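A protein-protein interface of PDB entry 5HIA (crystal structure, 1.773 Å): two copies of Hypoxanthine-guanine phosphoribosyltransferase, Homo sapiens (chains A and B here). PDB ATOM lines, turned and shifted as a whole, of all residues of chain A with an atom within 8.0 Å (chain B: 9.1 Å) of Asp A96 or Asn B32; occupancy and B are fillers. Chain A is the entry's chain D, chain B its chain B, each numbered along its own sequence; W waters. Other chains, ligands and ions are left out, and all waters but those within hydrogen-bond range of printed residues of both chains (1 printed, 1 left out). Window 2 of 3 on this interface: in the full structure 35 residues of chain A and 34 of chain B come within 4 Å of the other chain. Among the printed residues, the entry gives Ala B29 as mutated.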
ATOM      1  N   LEU A  91      22.206 -24.190 -18.530  1.00  0.00           N
ATOM      2  CA  LEU A  91      23.531 -24.579 -19.005  1.00  0.00           C
ATOM      3  C   LEU A  91      23.963 -23.745 -20.203  1.00  0.00           C
ATOM      4  O   LEU A  91      25.107 -23.301 -20.287  1.00  0.00           O
ATOM      5  CB  LEU A  91      23.565 -26.061 -19.383  1.00  0.00           C
ATOM      6  CG  LEU A  91      23.515 -27.031 -18.204  1.00  0.00           C
ATOM      7  CD1 LEU A  91      23.479 -28.462 -18.696  1.00  0.00           C
ATOM      8  CD2 LEU A  91      24.718 -26.806 -17.289  1.00  0.00           C
ATOM      9  N   ASN A  92      23.036 -23.538 -21.129  1.00  0.00           N
ATOM     10  CA  ASN A  92      23.353 -22.908 -22.396  1.00  0.00           C
ATOM     11  C   ASN A  92      23.628 -21.409 -22.321  1.00  0.00           C
ATOM     12  O   ASN A  92      24.188 -20.847 -23.262  1.00  0.00           O
ATOM     13  CB  ASN A  92      22.221 -23.171 -23.393  1.00  0.00           C
ATOM     14  CG  ASN A  92      22.364 -24.509 -24.096  1.00  0.00           C
ATOM     15  OD1 ASN A  92      23.026 -24.613 -25.129  1.00  0.00           O
ATOM     16  ND2 ASN A  92      21.735 -25.532 -23.550  1.00  0.00           N
ATOM     17  N   ARG A  93      23.236 -20.759 -21.228  1.00  0.00           N
ATOM     18  CA  ARG A  93      23.427 -19.308 -21.120  1.00  0.00           C
ATOM     19  C   ARG A  93      24.510 -18.959 -20.100  1.00  0.00           C
ATOM     20  O   ARG A  93      24.745 -17.792 -19.803  1.00  0.00           O
ATOM     21  CB  ARG A  93      22.107 -18.605 -20.762  1.00  0.00           C
ATOM     22  CG  ARG A  93      21.643 -18.811 -19.339  1.00  0.00           C
ATOM     23  CD  ARG A  93      20.371 -18.041 -19.020  1.00  0.00           C
ATOM     24  NE  ARG A  93      19.821 -18.498 -17.746  1.00  0.00           N
ATOM     25  CZ  ARG A  93      18.755 -19.286 -17.604  1.00  0.00           C
ATOM     26  NH1 ARG A  93      18.064 -19.717 -18.662  1.00  0.00           N
ATOM     27  NH2 ARG A  93      18.373 -19.650 -16.385  1.00  0.00           N
ATOM     28  N   ASN A  94      25.180 -19.978 -19.579  1.00  0.00           N
ATOM     29  CA  ASN A  94      26.250 -19.758 -18.625  1.00  0.00           C
ATOM     30  C   ASN A  94      27.508 -20.520 -19.014  1.00  0.00           C
ATOM     31  O   ASN A  94      28.462 -20.612 -18.243  1.00  0.00           O
ATOM     32  CB  ASN A  94      25.792 -20.147 -17.225  1.00  0.00           C
ATOM     33  CG  ASN A  94      24.816 -19.148 -16.641  1.00  0.00           C
ATOM     34  OD1 ASN A  94      25.189 -18.016 -16.323  1.00  0.00           O
ATOM     35  ND2 ASN A  94      23.563 -19.557 -16.494  1.00  0.00           N
ATOM     36  N   SER A  95      27.489 -21.055 -20.226  1.00  0.00           N
ATOM     37  CA  SER A  95      28.628 -21.761 -20.792  1.00  0.00           C
ATOM     38  C   SER A  95      29.136 -21.016 -22.016  1.00  0.00           C
ATOM     39  O   SER A  95      28.448 -20.147 -22.548  1.00  0.00           O
ATOM     40  CB  SER A  95      28.234 -23.183 -21.181  1.00  0.00           C
ATOM     41  OG  SER A  95      27.250 -23.149 -22.203  1.00  0.00           O
ATOM     42  N   ASP A  96      30.329 -21.369 -22.474  1.00  0.00           N
ATOM     43  CA  ASP A  96      30.841 -20.826 -23.721  1.00  0.00           C
ATOM     44  C   ASP A  96      30.105 -21.467 -24.893  1.00  0.00           C
ATOM     45  O   ASP A  96      29.570 -20.774 -25.761  1.00  0.00           O
ATOM     46  CB  ASP A  96      32.347 -21.057 -23.835  1.00  0.00           C
ATOM     47  CG  ASP A  96      33.130 -20.303 -22.774  1.00  0.00           C
ATOM     48  OD1 ASP A  96      32.581 -19.326 -22.221  1.00  0.00           O
ATOM     49  OD2 ASP A  96      34.288 -20.683 -22.493  1.00  0.00           O
ATOM     50  N   ARG A  97      30.061 -22.795 -24.898  1.00  0.00           N
ATOM     51  CA  ARG A  97      29.390 -23.535 -25.958  1.00  0.00           C
ATOM     52  C   ARG A  97      27.888 -23.671 -25.699  1.00  0.00           C
ATOM     53  O   ARG A  97      27.463 -24.027 -24.598  1.00  0.00           O
ATOM     54  CB  ARG A  97      30.025 -24.911 -26.119  1.00  0.00           C
ATOM     55  N   SER A  98      27.091 -23.370 -26.721  1.00  0.00           N
ATOM     56  CA  SER A  98      25.651 -23.616 -26.685  1.00  0.00           C
ATOM     57  C   SER A  98      25.173 -24.034 -28.070  1.00  0.00           C
ATOM     58  O   SER A  98      25.889 -23.892 -29.058  1.00  0.00           O
ATOM     59  CB  SER A  98      24.879 -22.384 -26.209  1.00  0.00           C
ATOM     60  OG  SER A  98      24.870 -21.376 -27.199  1.00  0.00           O
ATOM     61  N   ILE A  99      23.954 -24.546 -28.129  1.00  0.00           N
ATOM     62  CA  ILE A  99      23.374 -25.055 -29.362  1.00  0.00           C
ATOM     63  C   ILE A  99      21.893 -24.657 -29.422  1.00  0.00           C
ATOM     64  O   ILE A  99      21.235 -24.625 -28.388  1.00  0.00           O
ATOM     65  CB  ILE A  99      23.548 -26.603 -29.438  1.00  0.00           C
ATOM     66  CG1 ILE A  99      23.165 -27.143 -30.812  1.00  0.00           C
ATOM     67  CG2 ILE A  99      22.787 -27.314 -28.313  1.00  0.00           C
ATOM     68  CD1 ILE A  99      24.194 -26.874 -31.877  1.00  0.00           C
ATOM     69  N   PRO A 100      21.363 -24.358 -30.621  1.00  0.00           N
ATOM     70  CA  PRO A 100      19.931 -24.051 -30.632  1.00  0.00           C
ATOM     71  C   PRO A 100      19.072 -25.267 -30.281  1.00  0.00           C
ATOM     72  O   PRO A 100      19.460 -26.413 -30.510  1.00  0.00           O
ATOM     73  CB  PRO A 100      19.671 -23.588 -32.075  1.00  0.00           C
ATOM     74  CG  PRO A 100      20.847 -24.063 -32.864  1.00  0.00           C
ATOM     75  CD  PRO A 100      22.003 -24.060 -31.913  1.00  0.00           C
ATOM     76  N   PHE B  28      22.797  -9.199 -19.008  1.00  0.00           N
ATOM     77  CA  PHE B  28      22.101 -10.428 -18.651  1.00  0.00           C
ATOM     78  C   PHE B  28      22.848 -11.657 -19.137  1.00  0.00           C
ATOM     79  O   PHE B  28      23.801 -11.550 -19.910  1.00  0.00           O
ATOM     80  CB  PHE B  28      20.680 -10.416 -19.229  1.00  0.00           C
ATOM     81  CG  PHE B  28      19.810  -9.361 -18.630  1.00  0.00           C
ATOM     82  CD1 PHE B  28      19.113  -9.609 -17.459  1.00  0.00           C
ATOM     83  CD2 PHE B  28      19.733  -8.096 -19.199  1.00  0.00           C
ATOM     84  CE1 PHE B  28      18.331  -8.628 -16.877  1.00  0.00           C
ATOM     85  CE2 PHE B  28      18.951  -7.117 -18.627  1.00  0.00           C
ATOM     86  CZ  PHE B  28      18.244  -7.377 -17.470  1.00  0.00           C
ATOM     87  N   ALA B  29      22.407 -12.823 -18.666  1.00  0.00           N
ATOM     88  CA  ALA B  29      22.882 -14.093 -19.176  1.00  0.00           C
ATOM     89  C   ALA B  29      22.015 -14.483 -20.375  1.00  0.00           C
ATOM     90  O   ALA B  29      20.795 -14.564 -20.259  1.00  0.00           O
ATOM     91  CB  ALA B  29      22.822 -15.166 -18.095  1.00  0.00           C
ATOM     92  N   ILE B  30      22.661 -14.691 -21.520  1.00  0.00           N
ATOM     93  CA  ILE B  30      21.995 -14.880 -22.812  1.00  0.00           C
ATOM     94  C   ILE B  30      22.667 -16.050 -23.513  1.00  0.00           C
ATOM     95  O   ILE B  30      23.889 -16.093 -23.540  1.00  0.00           O
ATOM     96  CB  ILE B  30      22.120 -13.588 -23.701  1.00  0.00           C
ATOM     97  CG1 ILE B  30      21.402 -12.406 -23.051  1.00  0.00           C
ATOM     98  CG2 ILE B  30      21.645 -13.821 -25.145  1.00  0.00           C
ATOM     99  CD1 ILE B  30      19.935 -12.598 -22.878  1.00  0.00           C
ATOM    100  N   PRO B  31      21.887 -16.991 -24.082  1.00  0.00           N
ATOM    101  CA  PRO B  31      22.510 -18.089 -24.839  1.00  0.00           C
ATOM    102  C   PRO B  31      23.412 -17.556 -25.948  1.00  0.00           C
ATOM    103  O   PRO B  31      22.986 -16.684 -26.706  1.00  0.00           O
ATOM    104  CB  PRO B  31      21.325 -18.853 -25.442  1.00  0.00           C
ATOM    105  CG  PRO B  31      20.106 -18.294 -24.844  1.00  0.00           C
ATOM    106  CD  PRO B  31      20.415 -17.009 -24.161  1.00  0.00           C
ATOM    107  N   ASN B  32      24.639 -18.057 -26.039  1.00  0.00           N
ATOM    108  CA  ASN B  32      25.574 -17.545 -27.034  1.00  0.00           C
ATOM    109  C   ASN B  32      25.070 -17.684 -28.471  1.00  0.00           C
ATOM    110  O   ASN B  32      25.409 -16.864 -29.322  1.00  0.00           O
ATOM    111  CB  ASN B  32      26.934 -18.231 -26.910  1.00  0.00           C
ATOM    112  CG  ASN B  32      27.938 -17.714 -27.930  1.00  0.00           C
ATOM    113  OD1 ASN B  32      28.375 -16.560 -27.865  1.00  0.00           O
ATOM    114  ND2 ASN B  32      28.309 -18.565 -28.878  1.00  0.00           N
ATOM    115  N   HIS B  33      24.255 -18.698 -28.751  1.00  0.00           N
ATOM    116  CA  HIS B  33      23.852 -18.915 -30.136  1.00  0.00           C
ATOM    117  C   HIS B  33      22.840 -17.870 -30.605  1.00  0.00           C
ATOM    118  O   HIS B  33      22.522 -17.818 -31.794  1.00  0.00           O
ATOM    119  CB  HIS B  33      23.316 -20.341 -30.352  1.00  0.00           C
ATOM    120  CG  HIS B  33      22.134 -20.707 -29.506  1.00  0.00           C
ATOM    121  ND1 HIS B  33      22.256 -21.141 -28.203  1.00  0.00           N
ATOM    122  CD2 HIS B  33      20.814 -20.762 -29.798  1.00  0.00           C
ATOM    123  CE1 HIS B  33      21.059 -21.421 -27.719  1.00  0.00           C
ATOM    124  NE2 HIS B  33      20.164 -21.198 -28.665  1.00  0.00           N
ATOM    125  N   TYR B  34      22.376 -17.013 -29.694  1.00  0.00           N
ATOM    126  CA  TYR B  34      21.490 -15.908 -30.070  1.00  0.00           C
ATOM    127  C   TYR B  34      22.144 -14.543 -29.881  1.00  0.00           C
ATOM    128  O   TYR B  34      21.463 -13.520 -29.931  1.00  0.00           O
ATOM    129  CB  TYR B  34      20.198 -15.938 -29.262  1.00  0.00           C
ATOM    130  CG  TYR B  34      19.281 -17.091 -29.574  1.00  0.00           C
ATOM    131  CD1 TYR B  34      19.112 -17.542 -30.874  1.00  0.00           C
ATOM    132  CD2 TYR B  34      18.579 -17.736 -28.554  1.00  0.00           C
ATOM    133  CE1 TYR B  34      18.253 -18.608 -31.159  1.00  0.00           C
ATOM    134  CE2 TYR B  34      17.732 -18.789 -28.825  1.00  0.00           C
ATOM    135  CZ  TYR B  34      17.570 -19.223 -30.128  1.00  0.00           C
ATOM    136  OH  TYR B  34      16.724 -20.283 -30.398  1.00  0.00           O
ATOM    137  N   ALA B  35      23.457 -14.537 -29.667  1.00  0.00           N
ATOM    138  CA  ALA B  35      24.182 -13.326 -29.268  1.00  0.00           C
ATOM    139  C   ALA B  35      24.058 -12.170 -30.263  1.00  0.00           C
ATOM    140  O   ALA B  35      24.095 -10.993 -29.881  1.00  0.00           O
ATOM    141  CB  ALA B  35      25.654 -13.655 -29.048  1.00  0.00           C
ATOM    142  N   GLU B  36      23.936 -12.489 -31.543  1.00  0.00           N
ATOM    143  CA  GLU B  36      23.826 -11.439 -32.549  1.00  0.00           C
ATOM    144  C   GLU B  36      22.431 -11.382 -33.153  1.00  0.00           C
ATOM    145  O   GLU B  36      22.175 -10.609 -34.065  1.00  0.00           O
ATOM    146  CB  GLU B  36      24.876 -11.646 -33.636  1.00  0.00           C
ATOM    147  CG  GLU B  36      26.270 -11.226 -33.202  1.00  0.00           C
ATOM    148  CD  GLU B  36      27.355 -11.921 -33.988  1.00  0.00           C
ATOM    149  OE1 GLU B  36      27.618 -13.107 -33.704  1.00  0.00           O
ATOM    150  OE2 GLU B  36      27.944 -11.286 -34.889  1.00  0.00           O
ATOM    151  N   ASP B  37      21.526 -12.192 -32.618  1.00  0.00           N
ATOM    152  CA  ASP B  37      20.183 -12.305 -33.177  1.00  0.00           C
ATOM    153  C   ASP B  37      19.151 -11.492 -32.433  1.00  0.00           C
ATOM    154  O   ASP B  37      18.006 -11.402 -32.869  1.00  0.00           O
ATOM    155  CB  ASP B  37      19.744 -13.771 -33.192  1.00  0.00           C
ATOM    156  CG  ASP B  37      20.713 -14.649 -33.933  1.00  0.00           C
ATOM    157  OD1 ASP B  37      21.212 -14.214 -34.986  1.00  0.00           O
ATOM    158  OD2 ASP B  37      20.999 -15.762 -33.452  1.00  0.00           O
ATOM    159  N   LEU B  38      19.545 -10.932 -31.294  1.00  0.00           N
ATOM    160  CA  LEU B  38      18.633 -10.152 -30.464  1.00  0.00           C
ATOM    161  C   LEU B  38      19.075  -8.699 -30.401  1.00  0.00           C
ATOM    162  O   LEU B  38      20.263  -8.407 -30.485  1.00  0.00           O
ATOM    163  CB  LEU B  38      18.552 -10.737 -29.056  1.00  0.00           C
ATOM    164  CG  LEU B  38      18.098 -12.193 -29.062  1.00  0.00           C
ATOM    165  CD1 LEU B  38      18.293 -12.810 -27.693  1.00  0.00           C
ATOM    166  CD2 LEU B  38      16.641 -12.282 -29.553  1.00  0.00           C
ATOM    167  N   ASP B 207      13.765 -21.335 -26.750  1.00  0.00           N
ATOM    168  CA  ASP B 207      14.769 -21.697 -25.735  1.00  0.00           C
ATOM    169  C   ASP B 207      15.497 -20.469 -25.197  1.00  0.00           C
ATOM    170  O   ASP B 207      16.718 -20.450 -25.083  1.00  0.00           O
ATOM    171  CB  ASP B 207      15.794 -22.681 -26.310  1.00  0.00           C
ATOM    172  CG  ASP B 207      16.442 -22.168 -27.595  1.00  0.00           C
ATOM    173  OD1 ASP B 207      15.781 -21.383 -28.317  1.00  0.00           O
ATOM    174  OD2 ASP B 207      17.612 -22.526 -27.873  1.00  0.00           O
ATOM    175  N   LEU B 208      14.729 -19.441 -24.881  1.00  0.00           N
ATOM    176  CA  LEU B 208      15.264 -18.204 -24.347  1.00  0.00           C
ATOM    177  C   LEU B 208      14.376 -17.862 -23.164  1.00  0.00           C
ATOM    178  O   LEU B 208      13.146 -17.946 -23.291  1.00  0.00           O
ATOM    179  CB  LEU B 208      15.259 -17.109 -25.416  1.00  0.00           C
ATOM    180  CG  LEU B 208      15.555 -15.661 -25.022  1.00  0.00           C
ATOM    181  CD1 LEU B 208      16.951 -15.523 -24.419  1.00  0.00           C
ATOM    182  CD2 LEU B 208      15.391 -14.742 -26.223  1.00  0.00           C
ATOM    183  N   LYS B 221      18.639 -14.391 -40.434  1.00  0.00           N
ATOM    184  CA  LYS B 221      19.247 -15.701 -40.234  1.00  0.00           C
ATOM    185  C   LYS B 221      18.208 -16.818 -40.127  1.00  0.00           C
ATOM    186  O   LYS B 221      18.406 -17.901 -40.672  1.00  0.00           O
ATOM    187  CB  LYS B 221      20.127 -15.696 -38.979  1.00  0.00           C
ATOM    188  CG  LYS B 221      20.824 -17.029 -38.701  1.00  0.00           C
ATOM    189  CD  LYS B 221      21.555 -17.013 -37.355  1.00  0.00           C
ATOM    190  CE  LYS B 221      22.649 -15.959 -37.341  1.00  0.00           C
ATOM    191  NZ  LYS B 221      23.195 -15.724 -35.975  1.00  0.00           N
ATOM    192  N   TYR B 222      17.114 -16.552 -39.421  1.00  0.00           N
ATOM    193  CA  TYR B 222      16.115 -17.572 -39.129  1.00  0.00           C
ATOM    194  C   TYR B 222      14.877 -17.413 -40.008  1.00  0.00           C
ATOM    195  O   TYR B 222      13.833 -18.020 -39.753  1.00  0.00           O
ATOM    196  CB  TYR B 222      15.734 -17.530 -37.640  1.00  0.00           C
ATOM    197  CG  TYR B 222      16.919 -17.740 -36.719  1.00  0.00           C
ATOM    198  CD1 TYR B 222      17.626 -18.942 -36.720  1.00  0.00           C
ATOM    199  CD2 TYR B 222      17.329 -16.740 -35.844  1.00  0.00           C
ATOM    200  CE1 TYR B 222      18.718 -19.136 -35.871  1.00  0.00           C
ATOM    201  CE2 TYR B 222      18.421 -16.923 -34.997  1.00  0.00           C
ATOM    202  CZ  TYR B 222      19.111 -18.122 -35.014  1.00  0.00           C
ATOM    203  OH  TYR B 222      20.201 -18.302 -34.182  1.00  0.00           O
HETATM  204  O   HOH W   1      26.159 -19.501 -23.928  1.00  0.00           O
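A ring nitrogen (ND1) of His B33 lies within hydrogen-bond range of the side-chain hydroxyl (OG) of Ser A98 (2.8 Å).
NE2 of His B33 lies within hydrogen-bond range of OD2 of Asp B207 (3.0 Å). The backbone carbonyl oxygen (O) of His B33 lies within hydrogen-bond range of the side-chain hydroxyl (OH) of Tyr B222 (3.4 Å). OH of Tyr B34 lies within hydrogen-bond range of OD1 of Asp B207 (2.5 Å). OD1 of Asn A92 is in hydrogen-bond range of N of Ile A99 (3.1 Å).
Among the printed residues, pairs that only touch across the chains: Asn A92 with Pro B31 (3.6 Å), Asn A92 with Asn B32 (3.96 Å), Arg A93 with Ala B29 (3.7 Å), Arg A93 with Ile B30 (3.8 Å), Arg A93 with Pro B31 (3.7 Å), Asp A96 with Asn B32 (3.8 Å), Ser A98 with Asn B32 (3.5 Å), Ile A99 with His B33 (3.3 Å), Pro A100 with His B33 (3.5 Å) and Pro A100 with Asp B207 (3.9 Å).
Of the printed residues of chain B, Asp A96 touches Asn B32 (3.8 Å). No residue of chain B comes within 4 Å of Arg A97. Of the printed residues of chain A, Ile B30 touches Arg A93. Of the printed residues of chain B, Ile A99 touches His B33 (3.3 Å). Printed residues of chain A within 4 Å of Pro B31: Asn A92 (3.6 Å) and Arg A93 (3.7 Å). Printed residues of chain A within 4 Å of His B33: Ser A98, Ile A99 and Pro A100. The nearest residue of chain A that does not touch Asn B32 is Ser A95 (5.0 Å).
Of the 10 printed residues of chain A, 6 touch a printed residue of chain B. Printed residues of chain A that touch a printed residue of chain B: Asn A92, Arg A93, Asp A96, Ser A98, Ile A99 and Pro A100. Of the 15 printed residues of chain B, 6 touch a printed residue of chain A. Printed residues of chain B that touch a printed residue of chain A: Ala B29, Ile B30, Pro B31, Asn B32, His B33 and Asp B207. Among the printed residues, no Asp or Glu carboxylate lies within 4 Å of a Lys or Arg side-chain nitrogen of the other chain.
No position is printed for both chains. Of the 11 pairs that touch across the chains among the printed residues, none has its exchanged pair printed and touching as well.
Water W1 lies within hydrogen-bond range of O of Asn A92 (2.5 Å), O of Ser A95 (2.7 Å) and N of Asn B32 (3.0 Å).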
